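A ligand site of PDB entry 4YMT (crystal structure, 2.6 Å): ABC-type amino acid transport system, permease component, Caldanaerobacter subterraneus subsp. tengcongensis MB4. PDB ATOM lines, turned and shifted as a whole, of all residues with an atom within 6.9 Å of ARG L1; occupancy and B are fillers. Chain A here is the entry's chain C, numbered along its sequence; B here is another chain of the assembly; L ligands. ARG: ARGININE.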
ATOM      1  N   ILE A  62       5.742  32.862  -1.884  1.00  0.00           N
ATOM      2  CA  ILE A  62       5.405  31.499  -1.505  1.00  0.00           C
ATOM      3  C   ILE A  62       5.432  31.321   0.019  1.00  0.00           C
ATOM      4  O   ILE A  62       4.583  30.642   0.584  1.00  0.00           O
ATOM      5  CB  ILE A  62       6.366  30.486  -2.138  1.00  0.00           C
ATOM      6  CG1 ILE A  62       6.452  30.666  -3.657  1.00  0.00           C
ATOM      7  CG2 ILE A  62       5.964  29.055  -1.791  1.00  0.00           C
ATOM      8  CD1 ILE A  62       5.165  30.382  -4.372  1.00  0.00           C
ATOM      9  N   ARG A  63       6.397  31.938   0.694  1.00  0.00           N
ATOM     10  CA  ARG A  63       6.507  31.746   2.138  1.00  0.00           C
ATOM     11  C   ARG A  63       5.588  32.664   2.933  1.00  0.00           C
ATOM     12  O   ARG A  63       5.124  32.313   4.018  1.00  0.00           O
ATOM     13  CB  ARG A  63       7.955  31.923   2.583  1.00  0.00           C
ATOM     14  CG  ARG A  63       8.880  30.869   2.002  1.00  0.00           C
ATOM     15  CD  ARG A  63      10.311  31.047   2.469  1.00  0.00           C
ATOM     16  NE  ARG A  63      10.504  30.616   3.848  1.00  0.00           N
ATOM     17  CZ  ARG A  63      11.061  31.353   4.803  1.00  0.00           C
ATOM     18  NH1 ARG A  63      11.502  32.576   4.534  1.00  0.00           N
ATOM     19  NH2 ARG A  63      11.188  30.869   6.035  1.00  0.00           N
ATOM     20  N   GLY A  64       5.325  33.848   2.396  1.00  0.00           N
ATOM     21  CA  GLY A  64       4.546  34.809   3.146  1.00  0.00           C
ATOM     22  C   GLY A  64       3.056  34.597   2.977  1.00  0.00           C
ATOM     23  O   GLY A  64       2.233  35.380   3.454  1.00  0.00           O
ATOM     24  N   THR A  65       2.705  33.488   2.328  1.00  0.00           N
ATOM     25  CA  THR A  65       1.322  33.239   1.948  1.00  0.00           C
ATOM     26  C   THR A  65       0.949  31.756   2.166  1.00  0.00           C
ATOM     27  O   THR A  65       1.815  30.873   2.046  1.00  0.00           O
ATOM     28  CB  THR A  65       1.132  33.690   0.484  1.00  0.00           C
ATOM     29  OG1 THR A  65      -0.111  34.396   0.365  1.00  0.00           O
ATOM     30  CG2 THR A  65       1.221  32.521  -0.510  1.00  0.00           C
ATOM     31  N   PRO A  66      -0.331  31.468   2.523  1.00  0.00           N
ATOM     32  CA  PRO A  66      -0.754  30.126   2.961  1.00  0.00           C
ATOM     33  C   PRO A  66      -0.618  29.041   1.907  1.00  0.00           C
ATOM     34  O   PRO A  66      -0.785  29.339   0.740  1.00  0.00           O
ATOM     35  CB  PRO A  66      -2.233  30.324   3.319  1.00  0.00           C
ATOM     36  CG  PRO A  66      -2.396  31.773   3.574  1.00  0.00           C
ATOM     37  CD  PRO A  66      -1.443  32.430   2.602  1.00  0.00           C
ATOM     38  N   LEU A  67      -0.284  27.815   2.329  1.00  0.00           N
ATOM     39  CA  LEU A  67      -0.200  26.674   1.403  1.00  0.00           C
ATOM     40  C   LEU A  67      -1.583  26.372   0.776  1.00  0.00           C
ATOM     41  O   LEU A  67      -1.679  26.026  -0.403  1.00  0.00           O
ATOM     42  CB  LEU A  67       0.320  25.445   2.148  1.00  0.00           C
ATOM     43  CG  LEU A  67       1.088  24.303   1.449  1.00  0.00           C
ATOM     44  CD1 LEU A  67       0.736  22.995   2.117  1.00  0.00           C
ATOM     45  CD2 LEU A  67       0.878  24.202  -0.049  1.00  0.00           C
ATOM     46  N   LEU A  68      -2.631  26.479   1.602  1.00  0.00           N
ATOM     47  CA  LEU A  68      -4.007  26.217   1.191  1.00  0.00           C
ATOM     48  C   LEU A  68      -4.388  27.042  -0.030  1.00  0.00           C
ATOM     49  O   LEU A  68      -4.815  26.497  -1.052  1.00  0.00           O
ATOM     50  CB  LEU A  68      -4.989  26.521   2.335  1.00  0.00           C
ATOM     51  CG  LEU A  68      -6.197  25.584   2.487  1.00  0.00           C
ATOM     52  CD1 LEU A  68      -7.405  26.275   3.152  1.00  0.00           C
ATOM     53  CD2 LEU A  68      -6.607  24.924   1.184  1.00  0.00           C
ATOM     54  N   VAL A  69      -4.230  28.364   0.101  1.00  0.00           N
ATOM     55  CA  VAL A  69      -4.534  29.283  -0.982  1.00  0.00           C
ATOM     56  C   VAL A  69      -3.773  28.950  -2.255  1.00  0.00           C
ATOM     57  O   VAL A  69      -4.298  29.138  -3.337  1.00  0.00           O
ATOM     58  CB  VAL A  69      -4.253  30.736  -0.581  1.00  0.00           C
ATOM     59  CG1 VAL A  69      -4.502  31.688  -1.737  1.00  0.00           C
ATOM     60  CG2 VAL A  69      -5.078  31.114   0.653  1.00  0.00           C
ATOM     61  N   GLN A  70      -2.558  28.415  -2.118  1.00  0.00           N
ATOM     62  CA  GLN A  70      -1.763  28.029  -3.296  1.00  0.00           C
ATOM     63  C   GLN A  70      -2.358  26.778  -3.962  1.00  0.00           C
ATOM     64  O   GLN A  70      -2.436  26.684  -5.202  1.00  0.00           O
ATOM     65  CB  GLN A  70      -0.292  27.794  -2.902  1.00  0.00           C
ATOM     66  CG  GLN A  70       0.409  29.043  -2.413  1.00  0.00           C
ATOM     67  CD  GLN A  70       1.764  28.791  -1.736  1.00  0.00           C
ATOM     68  OE1 GLN A  70       2.207  29.591  -0.909  1.00  0.00           O
ATOM     69  NE2 GLN A  70       2.446  27.713  -2.128  1.00  0.00           N
ATOM     70  N   LEU A  95       2.469  21.465  -3.212  1.00  0.00           N
ATOM     71  CA  LEU A  95       3.427  21.110  -2.170  1.00  0.00           C
ATOM     72  C   LEU A  95       4.881  21.317  -2.619  1.00  0.00           C
ATOM     73  O   LEU A  95       5.666  21.868  -1.859  1.00  0.00           O
ATOM     74  CB  LEU A  95       3.210  19.669  -1.703  1.00  0.00           C
ATOM     75  CG  LEU A  95       1.956  19.302  -0.889  1.00  0.00           C
ATOM     76  CD1 LEU A  95       2.056  17.882  -0.344  1.00  0.00           C
ATOM     77  CD2 LEU A  95       1.645  20.281   0.245  1.00  0.00           C
ATOM     78  N   ILE A  97       5.952  23.379  -4.908  1.00  0.00           N
ATOM     79  CA  ILE A  97       6.184  24.794  -5.118  1.00  0.00           C
ATOM     80  C   ILE A  97       6.401  25.485  -3.764  1.00  0.00           C
ATOM     81  O   ILE A  97       7.241  26.375  -3.635  1.00  0.00           O
ATOM     82  CB  ILE A  97       4.995  25.439  -5.867  1.00  0.00           C
ATOM     83  CG1 ILE A  97       5.063  25.106  -7.355  1.00  0.00           C
ATOM     84  CG2 ILE A  97       4.966  26.949  -5.669  1.00  0.00           C
ATOM     85  CD1 ILE A  97       3.780  25.465  -8.109  1.00  0.00           C
ATOM     86  N   ASN A  98       5.649  25.067  -2.752  1.00  0.00           N
ATOM     87  CA  ASN A  98       5.812  25.592  -1.406  1.00  0.00           C
ATOM     88  C   ASN A  98       7.208  25.191  -0.834  1.00  0.00           C
ATOM     89  O   ASN A  98       8.001  26.023  -0.293  1.00  0.00           O
ATOM     90  CB  ASN A  98       4.663  25.065  -0.560  1.00  0.00           C
ATOM     91  CG  ASN A  98       4.578  25.716   0.789  1.00  0.00           C
ATOM     92  OD1 ASN A  98       4.889  25.095   1.793  1.00  0.00           O
ATOM     93  ND2 ASN A  98       4.128  26.956   0.819  1.00  0.00           N
ATOM     94  N   SER A  99       7.503  23.918  -1.032  1.00  0.00           N
ATOM     95  CA  SER A  99       8.741  23.317  -0.572  1.00  0.00           C
ATOM     96  C   SER A  99       9.935  23.942  -1.286  1.00  0.00           C
ATOM     97  O   SER A  99      11.002  24.074  -0.702  1.00  0.00           O
ATOM     98  CB  SER A  99       8.714  21.803  -0.802  1.00  0.00           C
ATOM     99  OG  SER A  99       9.904  21.171  -0.351  1.00  0.00           O
ATOM    100  N   SER A 100       9.768  24.332  -2.549  1.00  0.00           N
ATOM    101  CA  SER A 100      10.877  24.884  -3.302  1.00  0.00           C
ATOM    102  C   SER A 100      11.367  26.183  -2.660  1.00  0.00           C
ATOM    103  O   SER A 100      12.573  26.448  -2.605  1.00  0.00           O
ATOM    104  CB  SER A 100      10.474  25.150  -4.760  1.00  0.00           C
ATOM    105  OG  SER A 100       9.627  26.278  -4.833  1.00  0.00           O
ATOM    106  N   ALA A 101      10.438  26.998  -2.174  1.00  0.00           N
ATOM    107  CA  ALA A 101      10.822  28.270  -1.586  1.00  0.00           C
ATOM    108  C   ALA A 101      11.469  28.039  -0.227  1.00  0.00           C
ATOM    109  O   ALA A 101      12.540  28.621   0.103  1.00  0.00           O
ATOM    110  CB  ALA A 101       9.630  29.191  -1.469  1.00  0.00           C
ATOM    111  N   TYR A 102      10.868  27.149   0.562  1.00  0.00           N
ATOM    112  CA  TYR A 102      11.446  26.931   1.887  1.00  0.00           C
ATOM    113  C   TYR A 102      12.837  26.286   1.773  1.00  0.00           C
ATOM    114  O   TYR A 102      13.731  26.595   2.567  1.00  0.00           O
ATOM    115  CB  TYR A 102      10.512  26.092   2.774  1.00  0.00           C
ATOM    116  CG  TYR A 102       9.326  26.895   3.245  1.00  0.00           C
ATOM    117  CD1 TYR A 102       9.319  27.488   4.500  1.00  0.00           C
ATOM    118  CD2 TYR A 102       8.209  27.075   2.435  1.00  0.00           C
ATOM    119  CE1 TYR A 102       8.221  28.223   4.939  1.00  0.00           C
ATOM    120  CE2 TYR A 102       7.120  27.810   2.863  1.00  0.00           C
ATOM    121  CZ  TYR A 102       7.125  28.383   4.110  1.00  0.00           C
ATOM    122  OH  TYR A 102       6.055  29.120   4.525  1.00  0.00           O
ATOM    123  N   VAL A 103      13.025  25.424   0.780  1.00  0.00           N
ATOM    124  CA  VAL A 103      14.308  24.776   0.569  1.00  0.00           C
ATOM    125  C   VAL A 103      15.332  25.817   0.078  1.00  0.00           C
ATOM    126  O   VAL A 103      16.502  25.794   0.499  1.00  0.00           O
ATOM    127  CB  VAL A 103      14.199  23.618  -0.431  1.00  0.00           C
ATOM    128  CG1 VAL A 103      15.586  23.245  -0.974  1.00  0.00           C
ATOM    129  CG2 VAL A 103      13.564  22.410   0.249  1.00  0.00           C
ATOM    130  N   GLU A 152      12.593  19.234   6.709  1.00  0.00           N
ATOM    131  CA  GLU A 152      11.608  19.806   5.801  1.00  0.00           C
ATOM    132  C   GLU A 152      10.612  18.713   5.377  1.00  0.00           C
ATOM    133  O   GLU A 152       9.405  18.918   5.382  1.00  0.00           O
ATOM    134  CB  GLU A 152      12.300  20.431   4.581  1.00  0.00           C
ATOM    135  CG  GLU A 152      11.408  20.738   3.386  1.00  0.00           C
ATOM    136  CD  GLU A 152      10.453  21.886   3.629  1.00  0.00           C
ATOM    137  OE1 GLU A 152      10.509  22.501   4.721  1.00  0.00           O
ATOM    138  OE2 GLU A 152       9.641  22.186   2.731  1.00  0.00           O
ATOM    139  N   VAL A 155       8.219  17.915   8.246  1.00  0.00           N
ATOM    140  CA  VAL A 155       7.184  18.953   8.314  1.00  0.00           C
ATOM    141  C   VAL A 155       6.143  18.817   7.176  1.00  0.00           C
ATOM    142  O   VAL A 155       4.945  18.990   7.399  1.00  0.00           O
ATOM    143  CB  VAL A 155       7.816  20.358   8.287  1.00  0.00           C
ATOM    144  CG1 VAL A 155       6.775  21.448   8.051  1.00  0.00           C
ATOM    145  CG2 VAL A 155       8.544  20.607   9.581  1.00  0.00           C
ATOM    146  N   MET A 156       6.594  18.532   5.956  1.00  0.00           N
ATOM    147  CA  MET A 156       5.680  18.391   4.834  1.00  0.00           C
ATOM    148  C   MET A 156       4.710  17.203   4.983  1.00  0.00           C
ATOM    149  O   MET A 156       3.603  17.248   4.469  1.00  0.00           O
ATOM    150  CB  MET A 156       6.445  18.279   3.515  1.00  0.00           C
ATOM    151  CG  MET A 156       7.013  19.605   3.060  1.00  0.00           C
ATOM    152  SD  MET A 156       5.767  20.918   2.949  1.00  0.00           S
ATOM    153  CE  MET A 156       5.256  20.750   1.236  1.00  0.00           C
ATOM    154  N   GLU A 159       2.002  18.651   6.554  1.00  0.00           N
ATOM    155  CA  GLU A 159       1.418  19.619   5.634  1.00  0.00           C
ATOM    156  C   GLU A 159       0.559  18.960   4.544  1.00  0.00           C
ATOM    157  O   GLU A 159      -0.474  19.519   4.164  1.00  0.00           O
ATOM    158  CB  GLU A 159       2.536  20.443   4.981  1.00  0.00           C
ATOM    159  CG  GLU A 159       3.222  21.391   5.947  1.00  0.00           C
ATOM    160  CD  GLU A 159       2.390  22.630   6.222  1.00  0.00           C
ATOM    161  OE1 GLU A 159       1.741  23.119   5.272  1.00  0.00           O
ATOM    162  OE2 GLU A 159       2.346  23.110   7.377  1.00  0.00           O
ATOM    163  N   VAL B 155       2.761  33.351  11.813  1.00  0.00           N
ATOM    164  CA  VAL B 155       2.605  32.023  11.234  1.00  0.00           C
ATOM    165  C   VAL B 155       1.136  31.556  11.368  1.00  0.00           C
ATOM    166  O   VAL B 155       0.567  30.963  10.433  1.00  0.00           O
ATOM    167  CB  VAL B 155       3.558  31.013  11.908  1.00  0.00           C
ATOM    168  CG1 VAL B 155       3.246  29.591  11.476  1.00  0.00           C
ATOM    169  CG2 VAL B 155       4.974  31.349  11.557  1.00  0.00           C
ATOM    170  N   LYS B 158      -1.297  32.701   8.592  1.00  0.00           N
ATOM    171  CA  LYS B 158      -1.363  31.811   7.453  1.00  0.00           C
ATOM    172  C   LYS B 158      -2.116  30.542   7.842  1.00  0.00           C
ATOM    173  O   LYS B 158      -2.983  30.070   7.101  1.00  0.00           O
ATOM    174  CB  LYS B 158       0.030  31.483   6.933  1.00  0.00           C
ATOM    175  CG  LYS B 158       0.813  32.698   6.477  1.00  0.00           C
ATOM    176  CD  LYS B 158       2.085  32.289   5.750  1.00  0.00           C
ATOM    177  CE  LYS B 158       3.028  31.470   6.641  1.00  0.00           C
ATOM    178  NZ  LYS B 158       4.103  30.815   5.825  1.00  0.00           N
ATOM    179  N   GLU B 159      -1.823  30.013   9.028  1.00  0.00           N
ATOM    180  CA  GLU B 159      -2.415  28.752   9.466  1.00  0.00           C
ATOM    181  C   GLU B 159      -3.957  28.791   9.572  1.00  0.00           C
ATOM    182  O   GLU B 159      -4.607  27.781   9.345  1.00  0.00           O
ATOM    183  CB  GLU B 159      -1.809  28.336  10.808  1.00  0.00           C
ATOM    184  CG  GLU B 159      -0.329  27.957  10.712  1.00  0.00           C
ATOM    185  CD  GLU B 159      -0.092  26.605  10.065  1.00  0.00           C
ATOM    186  OE1 GLU B 159      -0.891  25.673  10.274  1.00  0.00           O
ATOM    187  OE2 GLU B 159       0.899  26.448   9.336  1.00  0.00           O
HETATM  188  N   ARG L   1       1.066  25.853   6.630  1.00  0.00           N
HETATM  189  CA  ARG L   1       1.843  27.085   6.550  1.00  0.00           C
HETATM  190  C   ARG L   1       1.431  27.926   5.341  1.00  0.00           C
HETATM  191  O   ARG L   1       1.995  29.004   5.109  1.00  0.00           O
HETATM  192  CB  ARG L   1       3.340  26.766   6.494  1.00  0.00           C
HETATM  193  CG  ARG L   1       3.812  26.050   5.247  1.00  0.00           C
HETATM  194  CD  ARG L   1       5.226  25.502   5.452  1.00  0.00           C
HETATM  195  NE  ARG L   1       5.826  25.097   4.190  1.00  0.00           N
HETATM  196  CZ  ARG L   1       6.934  24.366   4.086  1.00  0.00           C
HETATM  197  NH1 ARG L   1       7.416  24.049   2.888  1.00  0.00           N
HETATM  198  NH2 ARG L   1       7.562  23.953   5.180  1.00  0.00           N
HETATM  199  OXT ARG L   1       0.523  27.546   4.581  1.00  0.00           O
HETATM  200  N   ARG L   2       0.713  23.514   9.571  1.00  0.00           N
HETATM  201  CA  ARG L   2       1.595  22.672  10.372  1.00  0.00           C
HETATM  202  C   ARG L   2       0.846  21.534  11.056  1.00  0.00           C
HETATM  203  O   ARG L   2      -0.330  21.297  10.768  1.00  0.00           O
HETATM  204  CB  ARG L   2       2.323  23.504  11.412  1.00  0.00           C
HETATM  205  CG  ARG L   2       1.440  24.104  12.466  1.00  0.00           C
HETATM  206  CD  ARG L   2       2.230  25.161  13.238  1.00  0.00           C
HETATM  207  NE  ARG L   2       1.526  25.590  14.448  1.00  0.00           N
HETATM  208  CZ  ARG L   2       1.862  26.663  15.166  1.00  0.00           C
HETATM  209  NH1 ARG L   2       2.897  27.405  14.802  1.00  0.00           N
HETATM  210  NH2 ARG L   2       1.168  26.975  16.250  1.00  0.00           N
HETATM  211  OXT ARG L   2       1.384  20.826  11.911  1.00  0.00           O
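The side-chain carboxylate (OE1) of Glu 159 of chain B lies within salt-bridge range of a nitrogen (N) of ARG L2. The side-chain amide oxygen (OD1) of Asn 98 lies within hydrogen-bond range of a nitrogen (NE) of ARG L1, at 2.6 Å. NZ of Lys 158 of chain B is in salt-bridge range of O of ARG L1 (2.9 Å). The backbone NH of Leu 67 lies within hydrogen-bond range of an oxygen (OXT) of ARG L1. The side-chain carboxylate (OE2) of Glu 152 lies within salt-bridge range of a nitrogen (NH1) of ARG L1 (2.9 Å). The side-chain carboxylate of Glu 159 of chain B lies within salt-bridge range of a nitrogen (N) of ARG L1, at 2.8 Å. SD of Met 156 lies within hydrogen-bond range of NH1 of ARG L1 (3.5 Å). The side-chain carboxylate of Glu 159 of chain A is in salt-bridge range of a nitrogen (N) of ARG L1 (3.1 Å). OE2 of Glu 159 of chain A is in salt-bridge range of N of ARG L2 (2.8 Å).
ND2 of Asn 98 lies close to NE2 of Gln 70, at 3.5 Å. The backbone carbonyl oxygen (O) of Arg 63 lies within hydrogen-bond range of the side-chain hydroxyl (OH) of Tyr 102, 3.4 Å away. O of Arg 63 sits at hydrogen-bond distance from NZ of Lys 158 of chain B (2.6 Å). O of Thr 65 sits close to OE1 of Gln 70 (3.2 Å). The side-chain hydroxyl (OH) of Tyr 102 lies within hydrogen-bond range of the side-chain amino group (NZ) of Lys 158 of chain B (2.9 Å). OE2 of Glu 152 sits at hydrogen-bond distance from OG of Ser 99. O of Pro 66 lies close to OE1 of Gln 70 (3.4 Å).
Thr 65 touches ARG L1. C of Pro 66 touches OXT of ARG L1 (3.3 Å). Ser 99 touches ARG L1. CD2 of Tyr 102 touches NH1 of ARG L1, at 3.2 Å. Val 155 of chain A touches ARG L1 (CG1 to NH2, 3.9 Å). Hydrophobic or aromatic side chains within 4 Å of ARG L1: Leu 67, Tyr 102, Val 155 of chain A and Met 156.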
